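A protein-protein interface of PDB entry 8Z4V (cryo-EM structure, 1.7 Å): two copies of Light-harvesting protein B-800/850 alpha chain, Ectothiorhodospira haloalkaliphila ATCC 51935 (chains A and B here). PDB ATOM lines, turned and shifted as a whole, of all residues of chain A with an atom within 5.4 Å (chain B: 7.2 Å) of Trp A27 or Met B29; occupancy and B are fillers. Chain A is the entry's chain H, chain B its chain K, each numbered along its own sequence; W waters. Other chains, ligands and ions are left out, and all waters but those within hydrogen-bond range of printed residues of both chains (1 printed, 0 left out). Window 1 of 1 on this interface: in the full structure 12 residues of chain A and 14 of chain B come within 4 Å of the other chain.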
ATOM      1  N   VAL A  22      26.084   5.733   6.927  1.00  0.00           N
ATOM      2  CA  VAL A  22      26.658   7.083   7.136  1.00  0.00           C
ATOM      3  C   VAL A  22      26.701   7.300   8.642  1.00  0.00           C
ATOM      4  O   VAL A  22      25.648   7.305   9.244  1.00  0.00           O
ATOM      5  CB  VAL A  22      25.797   8.139   6.424  1.00  0.00           C
ATOM      6  CG1 VAL A  22      26.224   9.545   6.808  1.00  0.00           C
ATOM      7  CG2 VAL A  22      25.845   7.944   4.913  1.00  0.00           C
ATOM      8  N   ASN A  23      27.882   7.478   9.214  1.00  0.00           N
ATOM      9  CA  ASN A  23      28.012   7.725  10.664  1.00  0.00           C
ATOM     10  C   ASN A  23      27.706   9.206  10.884  1.00  0.00           C
ATOM     11  O   ASN A  23      28.430  10.056  10.376  1.00  0.00           O
ATOM     12  CB  ASN A  23      29.395   7.355  11.187  1.00  0.00           C
ATOM     13  CG  ASN A  23      29.446   7.419  12.701  1.00  0.00           C
ATOM     14  OD1 ASN A  23      28.844   8.289  13.318  1.00  0.00           O
ATOM     15  ND2 ASN A  23      30.084   6.447  13.325  1.00  0.00           N
ATOM     16  N   PRO A  24      26.612   9.548  11.589  1.00  0.00           N
ATOM     17  CA  PRO A  24      26.238  10.948  11.783  1.00  0.00           C
ATOM     18  C   PRO A  24      27.244  11.684  12.679  1.00  0.00           C
ATOM     19  O   PRO A  24      27.349  12.890  12.565  1.00  0.00           O
ATOM     20  CB  PRO A  24      24.839  10.898  12.406  1.00  0.00           C
ATOM     21  CG  PRO A  24      24.684   9.514  12.949  1.00  0.00           C
ATOM     22  CD  PRO A  24      25.675   8.620  12.225  1.00  0.00           C
ATOM     23  N   GLY A  25      28.004  10.945  13.493  1.00  0.00           N
ATOM     24  CA  GLY A  25      29.140  11.498  14.247  1.00  0.00           C
ATOM     25  C   GLY A  25      30.104  12.198  13.315  1.00  0.00           C
ATOM     26  O   GLY A  25      30.558  13.282  13.634  1.00  0.00           O
ATOM     27  N   THR A  26      30.361  11.616  12.151  1.00  0.00           N
ATOM     28  CA  THR A  26      31.266  12.185  11.137  1.00  0.00           C
ATOM     29  C   THR A  26      30.495  13.149  10.244  1.00  0.00           C
ATOM     30  O   THR A  26      31.060  14.186   9.883  1.00  0.00           O
ATOM     31  CB  THR A  26      31.865  11.071  10.277  1.00  0.00           C
ATOM     32  OG1 THR A  26      32.515  10.179  11.179  1.00  0.00           O
ATOM     33  CG2 THR A  26      32.835  11.592   9.243  1.00  0.00           C
ATOM     34  N   TRP A  27      29.276  12.787   9.842  1.00  0.00           N
ATOM     35  CA  TRP A  27      28.648  13.425   8.658  1.00  0.00           C
ATOM     36  C   TRP A  27      27.534  14.405   8.996  1.00  0.00           C
ATOM     37  O   TRP A  27      27.180  15.171   8.085  1.00  0.00           O
ATOM     38  CB  TRP A  27      28.168  12.347   7.694  1.00  0.00           C
ATOM     39  CG  TRP A  27      29.332  11.663   7.068  1.00  0.00           C
ATOM     40  CD1 TRP A  27      29.801  10.414   7.340  1.00  0.00           C
ATOM     41  CD2 TRP A  27      30.240  12.249   6.126  1.00  0.00           C
ATOM     42  NE1 TRP A  27      30.917  10.167   6.584  1.00  0.00           N
ATOM     43  CE2 TRP A  27      31.217  11.273   5.843  1.00  0.00           C
ATOM     44  CE3 TRP A  27      30.314  13.491   5.487  1.00  0.00           C
ATOM     45  CZ2 TRP A  27      32.261  11.513   4.948  1.00  0.00           C
ATOM     46  CZ3 TRP A  27      31.342  13.723   4.597  1.00  0.00           C
ATOM     47  CH2 TRP A  27      32.293  12.740   4.329  1.00  0.00           C
ATOM     48  N   LEU A  28      26.987  14.417  10.207  1.00  0.00           N
ATOM     49  CA  LEU A  28      25.849  15.333  10.436  1.00  0.00           C
ATOM     50  C   LEU A  28      26.314  16.777  10.203  1.00  0.00           C
ATOM     51  O   LEU A  28      25.629  17.495   9.467  1.00  0.00           O
ATOM     52  CB  LEU A  28      25.257  15.165  11.832  1.00  0.00           C
ATOM     53  CG  LEU A  28      24.103  16.119  12.133  1.00  0.00           C
ATOM     54  CD1 LEU A  28      22.973  15.955  11.115  1.00  0.00           C
ATOM     55  CD2 LEU A  28      23.600  15.900  13.542  1.00  0.00           C
ATOM     56  N   MET A  29      27.431  17.203  10.790  1.00  0.00           N
ATOM     57  CA  MET A  29      27.820  18.631  10.660  1.00  0.00           C
ATOM     58  C   MET A  29      28.133  18.955   9.199  1.00  0.00           C
ATOM     59  O   MET A  29      27.624  19.952   8.684  1.00  0.00           O
ATOM     60  CB  MET A  29      28.972  19.011  11.595  1.00  0.00           C
ATOM     61  CG  MET A  29      28.588  18.916  13.052  1.00  0.00           C
ATOM     62  SD  MET A  29      26.990  19.694  13.441  1.00  0.00           S
ATOM     63  CE  MET A  29      27.236  21.315  12.732  1.00  0.00           C
ATOM     64  N   PRO A  30      28.902  18.123   8.460  1.00  0.00           N
ATOM     65  CA  PRO A  30      29.089  18.354   7.027  1.00  0.00           C
ATOM     66  C   PRO A  30      27.764  18.430   6.263  1.00  0.00           C
ATOM     67  O   PRO A  30      27.636  19.297   5.437  1.00  0.00           O
ATOM     68  CB  PRO A  30      29.916  17.147   6.565  1.00  0.00           C
ATOM     69  CG  PRO A  30      30.692  16.778   7.802  1.00  0.00           C
ATOM     70  CD  PRO A  30      29.719  16.997   8.944  1.00  0.00           C
ATOM     71  N   ILE A  31      26.794  17.574   6.586  1.00  0.00           N
ATOM     72  CA  ILE A  31      25.460  17.648   5.925  1.00  0.00           C
ATOM     73  C   ILE A  31      24.860  19.036   6.176  1.00  0.00           C
ATOM     74  O   ILE A  31      24.419  19.676   5.212  1.00  0.00           O
ATOM     75  CB  ILE A  31      24.522  16.522   6.389  1.00  0.00           C
ATOM     76  CG1 ILE A  31      24.952  15.182   5.793  1.00  0.00           C
ATOM     77  CG2 ILE A  31      23.077  16.840   6.031  1.00  0.00           C
ATOM     78  CD1 ILE A  31      24.346  13.983   6.503  1.00  0.00           C
ATOM     79  N   LEU A  32      24.847  19.478   7.426  1.00  0.00           N
ATOM     80  CA  LEU A  32      24.226  20.774   7.788  1.00  0.00           C
ATOM     81  C   LEU A  32      25.011  21.920   7.144  1.00  0.00           C
ATOM     82  O   LEU A  32      24.366  22.868   6.655  1.00  0.00           O
ATOM     83  CB  LEU A  32      24.156  20.906   9.306  1.00  0.00           C
ATOM     84  CG  LEU A  32      23.241  19.888   9.993  1.00  0.00           C
ATOM     85  CD1 LEU A  32      23.151  20.175  11.477  1.00  0.00           C
ATOM     86  CD2 LEU A  32      21.852  19.871   9.376  1.00  0.00           C
ATOM     87  N   PRO B  24      30.974   3.123   1.003  1.00  0.00           N
ATOM     88  CA  PRO B  24      29.949   4.167   1.013  1.00  0.00           C
ATOM     89  C   PRO B  24      29.886   4.884   2.370  1.00  0.00           C
ATOM     90  O   PRO B  24      29.456   6.020   2.405  1.00  0.00           O
ATOM     91  CB  PRO B  24      28.642   3.437   0.683  1.00  0.00           C
ATOM     92  CG  PRO B  24      28.904   1.990   0.955  1.00  0.00           C
ATOM     93  CD  PRO B  24      30.405   1.777   0.911  1.00  0.00           C
ATOM     94  N   GLY B  25      30.375   4.240   3.433  1.00  0.00           N
ATOM     95  CA  GLY B  25      30.562   4.886   4.742  1.00  0.00           C
ATOM     96  C   GLY B  25      31.404   6.133   4.600  1.00  0.00           C
ATOM     97  O   GLY B  25      31.066   7.149   5.183  1.00  0.00           O
ATOM     98  N   THR B  26      32.448   6.078   3.784  1.00  0.00           N
ATOM     99  CA  THR B  26      33.351   7.216   3.534  1.00  0.00           C
ATOM    100  C   THR B  26      32.789   8.080   2.412  1.00  0.00           C
ATOM    101  O   THR B  26      32.897   9.307   2.512  1.00  0.00           O
ATOM    102  CB  THR B  26      34.740   6.715   3.136  1.00  0.00           C
ATOM    103  OG1 THR B  26      35.175   5.869   4.197  1.00  0.00           O
ATOM    104  CG2 THR B  26      35.721   7.839   2.905  1.00  0.00           C
ATOM    105  N   TRP B  27      32.274   7.463   1.347  1.00  0.00           N
ATOM    106  CA  TRP B  27      32.114   8.180   0.059  1.00  0.00           C
ATOM    107  C   TRP B  27      30.676   8.550  -0.275  1.00  0.00           C
ATOM    108  O   TRP B  27      30.518   9.391  -1.175  1.00  0.00           O
ATOM    109  CB  TRP B  27      32.754   7.366  -1.058  1.00  0.00           C
ATOM    110  CG  TRP B  27      34.235   7.367  -0.912  1.00  0.00           C
ATOM    111  CD1 TRP B  27      35.024   6.342  -0.484  1.00  0.00           C
ATOM    112  CD2 TRP B  27      35.094   8.499  -1.102  1.00  0.00           C
ATOM    113  NE1 TRP B  27      36.330   6.752  -0.446  1.00  0.00           N
ATOM    114  CE2 TRP B  27      36.404   8.069  -0.804  1.00  0.00           C
ATOM    115  CE3 TRP B  27      34.889   9.822  -1.505  1.00  0.00           C
ATOM    116  CZ2 TRP B  27      37.500   8.926  -0.893  1.00  0.00           C
ATOM    117  CZ3 TRP B  27      35.976  10.666  -1.602  1.00  0.00           C
ATOM    118  CH2 TRP B  27      37.261  10.215  -1.309  1.00  0.00           C
ATOM    119  N   LEU B  28      29.664   7.986   0.377  1.00  0.00           N
ATOM    120  CA  LEU B  28      28.292   8.326  -0.061  1.00  0.00           C
ATOM    121  C   LEU B  28      28.074   9.836   0.105  1.00  0.00           C
ATOM    122  O   LEU B  28      27.609  10.463  -0.853  1.00  0.00           O
ATOM    123  CB  LEU B  28      27.239   7.532   0.703  1.00  0.00           C
ATOM    124  CG  LEU B  28      25.803   7.875   0.316  1.00  0.00           C
ATOM    125  CD1 LEU B  28      25.568   7.658  -1.180  1.00  0.00           C
ATOM    126  CD2 LEU B  28      24.831   7.063   1.141  1.00  0.00           C
ATOM    127  N   MET B  29      28.393  10.416   1.261  1.00  0.00           N
ATOM    128  CA  MET B  29      28.073  11.853   1.464  1.00  0.00           C
ATOM    129  C   MET B  29      28.883  12.710   0.491  1.00  0.00           C
ATOM    130  O   MET B  29      28.306  13.576  -0.170  1.00  0.00           O
ATOM    131  CB  MET B  29      28.263  12.294   2.918  1.00  0.00           C
ATOM    132  CG  MET B  29      27.297  11.616   3.860  1.00  0.00           C
ATOM    133  SD  MET B  29      25.577  11.621   3.271  1.00  0.00           S
ATOM    134  CE  MET B  29      25.352  13.360   2.933  1.00  0.00           C
ATOM    135  N   PRO B  30      30.203  12.477   0.306  1.00  0.00           N
ATOM    136  CA  PRO B  30      30.951  13.200  -0.724  1.00  0.00           C
ATOM    137  C   PRO B  30      30.335  13.045  -2.118  1.00  0.00           C
ATOM    138  O   PRO B  30      30.252  14.027  -2.811  1.00  0.00           O
ATOM    139  CB  PRO B  30      32.349  12.569  -0.673  1.00  0.00           C
ATOM    140  CG  PRO B  30      32.464  12.123   0.761  1.00  0.00           C
ATOM    141  CD  PRO B  30      31.081  11.615   1.116  1.00  0.00           C
ATOM    142  N   ILE B  31      29.868  11.850  -2.479  1.00  0.00           N
ATOM    143  CA  ILE B  31      29.195  11.659  -3.796  1.00  0.00           C
ATOM    144  C   ILE B  31      27.985  12.595  -3.872  1.00  0.00           C
ATOM    145  O   ILE B  31      27.849  13.311  -4.874  1.00  0.00           O
ATOM    146  CB  ILE B  31      28.808  10.192  -4.039  1.00  0.00           C
ATOM    147  CG1 ILE B  31      30.046   9.347  -4.336  1.00  0.00           C
ATOM    148  CG2 ILE B  31      27.788  10.083  -5.164  1.00  0.00           C
ATOM    149  CD1 ILE B  31      29.808   7.854  -4.188  1.00  0.00           C
ATOM    150  N   LEU B  32      27.141  12.585  -2.850  1.00  0.00           N
ATOM    151  CA  LEU B  32      25.900  13.398  -2.855  1.00  0.00           C
ATOM    152  C   LEU B  32      26.259  14.887  -2.846  1.00  0.00           C
ATOM    153  O   LEU B  32      25.593  15.652  -3.571  1.00  0.00           O
ATOM    154  CB  LEU B  32      25.025  13.010  -1.666  1.00  0.00           C
ATOM    155  CG  LEU B  32      24.490  11.576  -1.711  1.00  0.00           C
ATOM    156  CD1 LEU B  32      23.545  11.330  -0.554  1.00  0.00           C
ATOM    157  CD2 LEU B  32      23.798  11.271  -3.029  1.00  0.00           C
ATOM    158  N   MET B  33      27.303  15.274  -2.122  1.00  0.00           N
ATOM    159  CA  MET B  33      27.748  16.685  -2.105  1.00  0.00           C
ATOM    160  C   MET B  33      28.266  17.058  -3.499  1.00  0.00           C
ATOM    161  O   MET B  33      27.904  18.142  -3.981  1.00  0.00           O
ATOM    162  CB  MET B  33      28.807  16.916  -1.027  1.00  0.00           C
ATOM    163  CG  MET B  33      28.231  16.768   0.372  1.00  0.00           C
ATOM    164  SD  MET B  33      29.531  16.647   1.620  1.00  0.00           S
ATOM    165  CE  MET B  33      28.526  16.607   3.105  1.00  0.00           C
ATOM    166  N   ALA B  34      28.989  16.159  -4.169  1.00  0.00           N
ATOM    167  CA  ALA B  34      29.503  16.407  -5.533  1.00  0.00           C
ATOM    168  C   ALA B  34      28.309  16.668  -6.455  1.00  0.00           C
ATOM    169  O   ALA B  34      28.357  17.637  -7.221  1.00  0.00           O
ATOM    170  CB  ALA B  34      30.351  15.251  -6.033  1.00  0.00           C
ATOM    171  N   VAL B  35      27.265  15.862  -6.343  1.00  0.00           N
ATOM    172  CA  VAL B  35      26.066  15.995  -7.212  1.00  0.00           C
ATOM    173  C   VAL B  35      25.374  17.330  -6.893  1.00  0.00           C
ATOM    174  O   VAL B  35      24.960  18.027  -7.844  1.00  0.00           O
ATOM    175  CB  VAL B  35      25.139  14.780  -7.063  1.00  0.00           C
ATOM    176  CG1 VAL B  35      23.882  14.939  -7.902  1.00  0.00           C
ATOM    177  CG2 VAL B  35      25.868  13.501  -7.462  1.00  0.00           C
HETATM  178  O   HOH W   1      30.339   7.018   7.757  1.00  0.00           O
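Of the 12 printed residues of chain B, 5 touch a printed residue of chain A.
Hydrophobic or aromatic side chains of chain B that line the printed part of chain A: Met B29, Pro B30 and Met B33.
Hydrophobic or aromatic side chains of chain A that line the printed part of chain B: Val A22, Trp A27, Pro A30 and Ile A31.
Printed residues of chain B within 4 Å of Val A22: Met B29.
Trp A27 touches four residues of chain B.
Leu A28 touches none of the printed residues of chain B.
Met A29 touches none of the printed residues of chain B.
Printed residues of chain B within 4 Å of Ile A31: Met B29.
Of the printed residues of chain A, Thr B26 touches Trp A27.
Met B29 touches just these residues of chain A: Val A22, Trp A27 and Ile A31.
The nearest printed residue of chain A that does not touch Met B29 is Pro A30 (6.3 Å).
The nearest printed residue of chain A that does not touch Gly B25 is Val A22 (4.8 Å).
Water W1 lies within hydrogen-bond range of the backbone carbonyl oxygen (O) of Gly B25 (2.7 Å), the backbone NH (N) of Asn A23 (2.9 Å) and the indole nitrogen (NE1) of Trp A27 (3.4 Å).
Among the printed residues, merely in contact across the chains: Trp A27 with Thr B26 (3.3 Å), Ile A31 with Met B29 (3.4 Å), Trp A27 with Met B29 (3.5 Å), Trp A27 with Pro B30 (3.6 Å), Pro A30 with Met B33 (3.7 Å) and Val A22 with Met B29 (3.8 Å).
NE1 of Trp A27 is in hydrogen-bond range of O of Gly B25, at 3.3 Å.
Trp A27 touches Thr B26, but with the chains exchanged Thr A26 does not touch Trp B27 (8.9 Å).
Trp A27 touches Met B29, but with the chains exchanged Met A29 does not touch Trp B27 (14.3 Å).
Trp A27 touches Pro B30, but with the chains exchanged Pro A30 does not touch Trp B27 (11.0 Å).
Ile A31 touches Met B29, but with the chains exchanged Met A29 does not touch Ile B31 (13.8 Å).
Of the 7 pairs that touch across the chains among the printed residues, none has its exchanged pair printed and touching as well.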
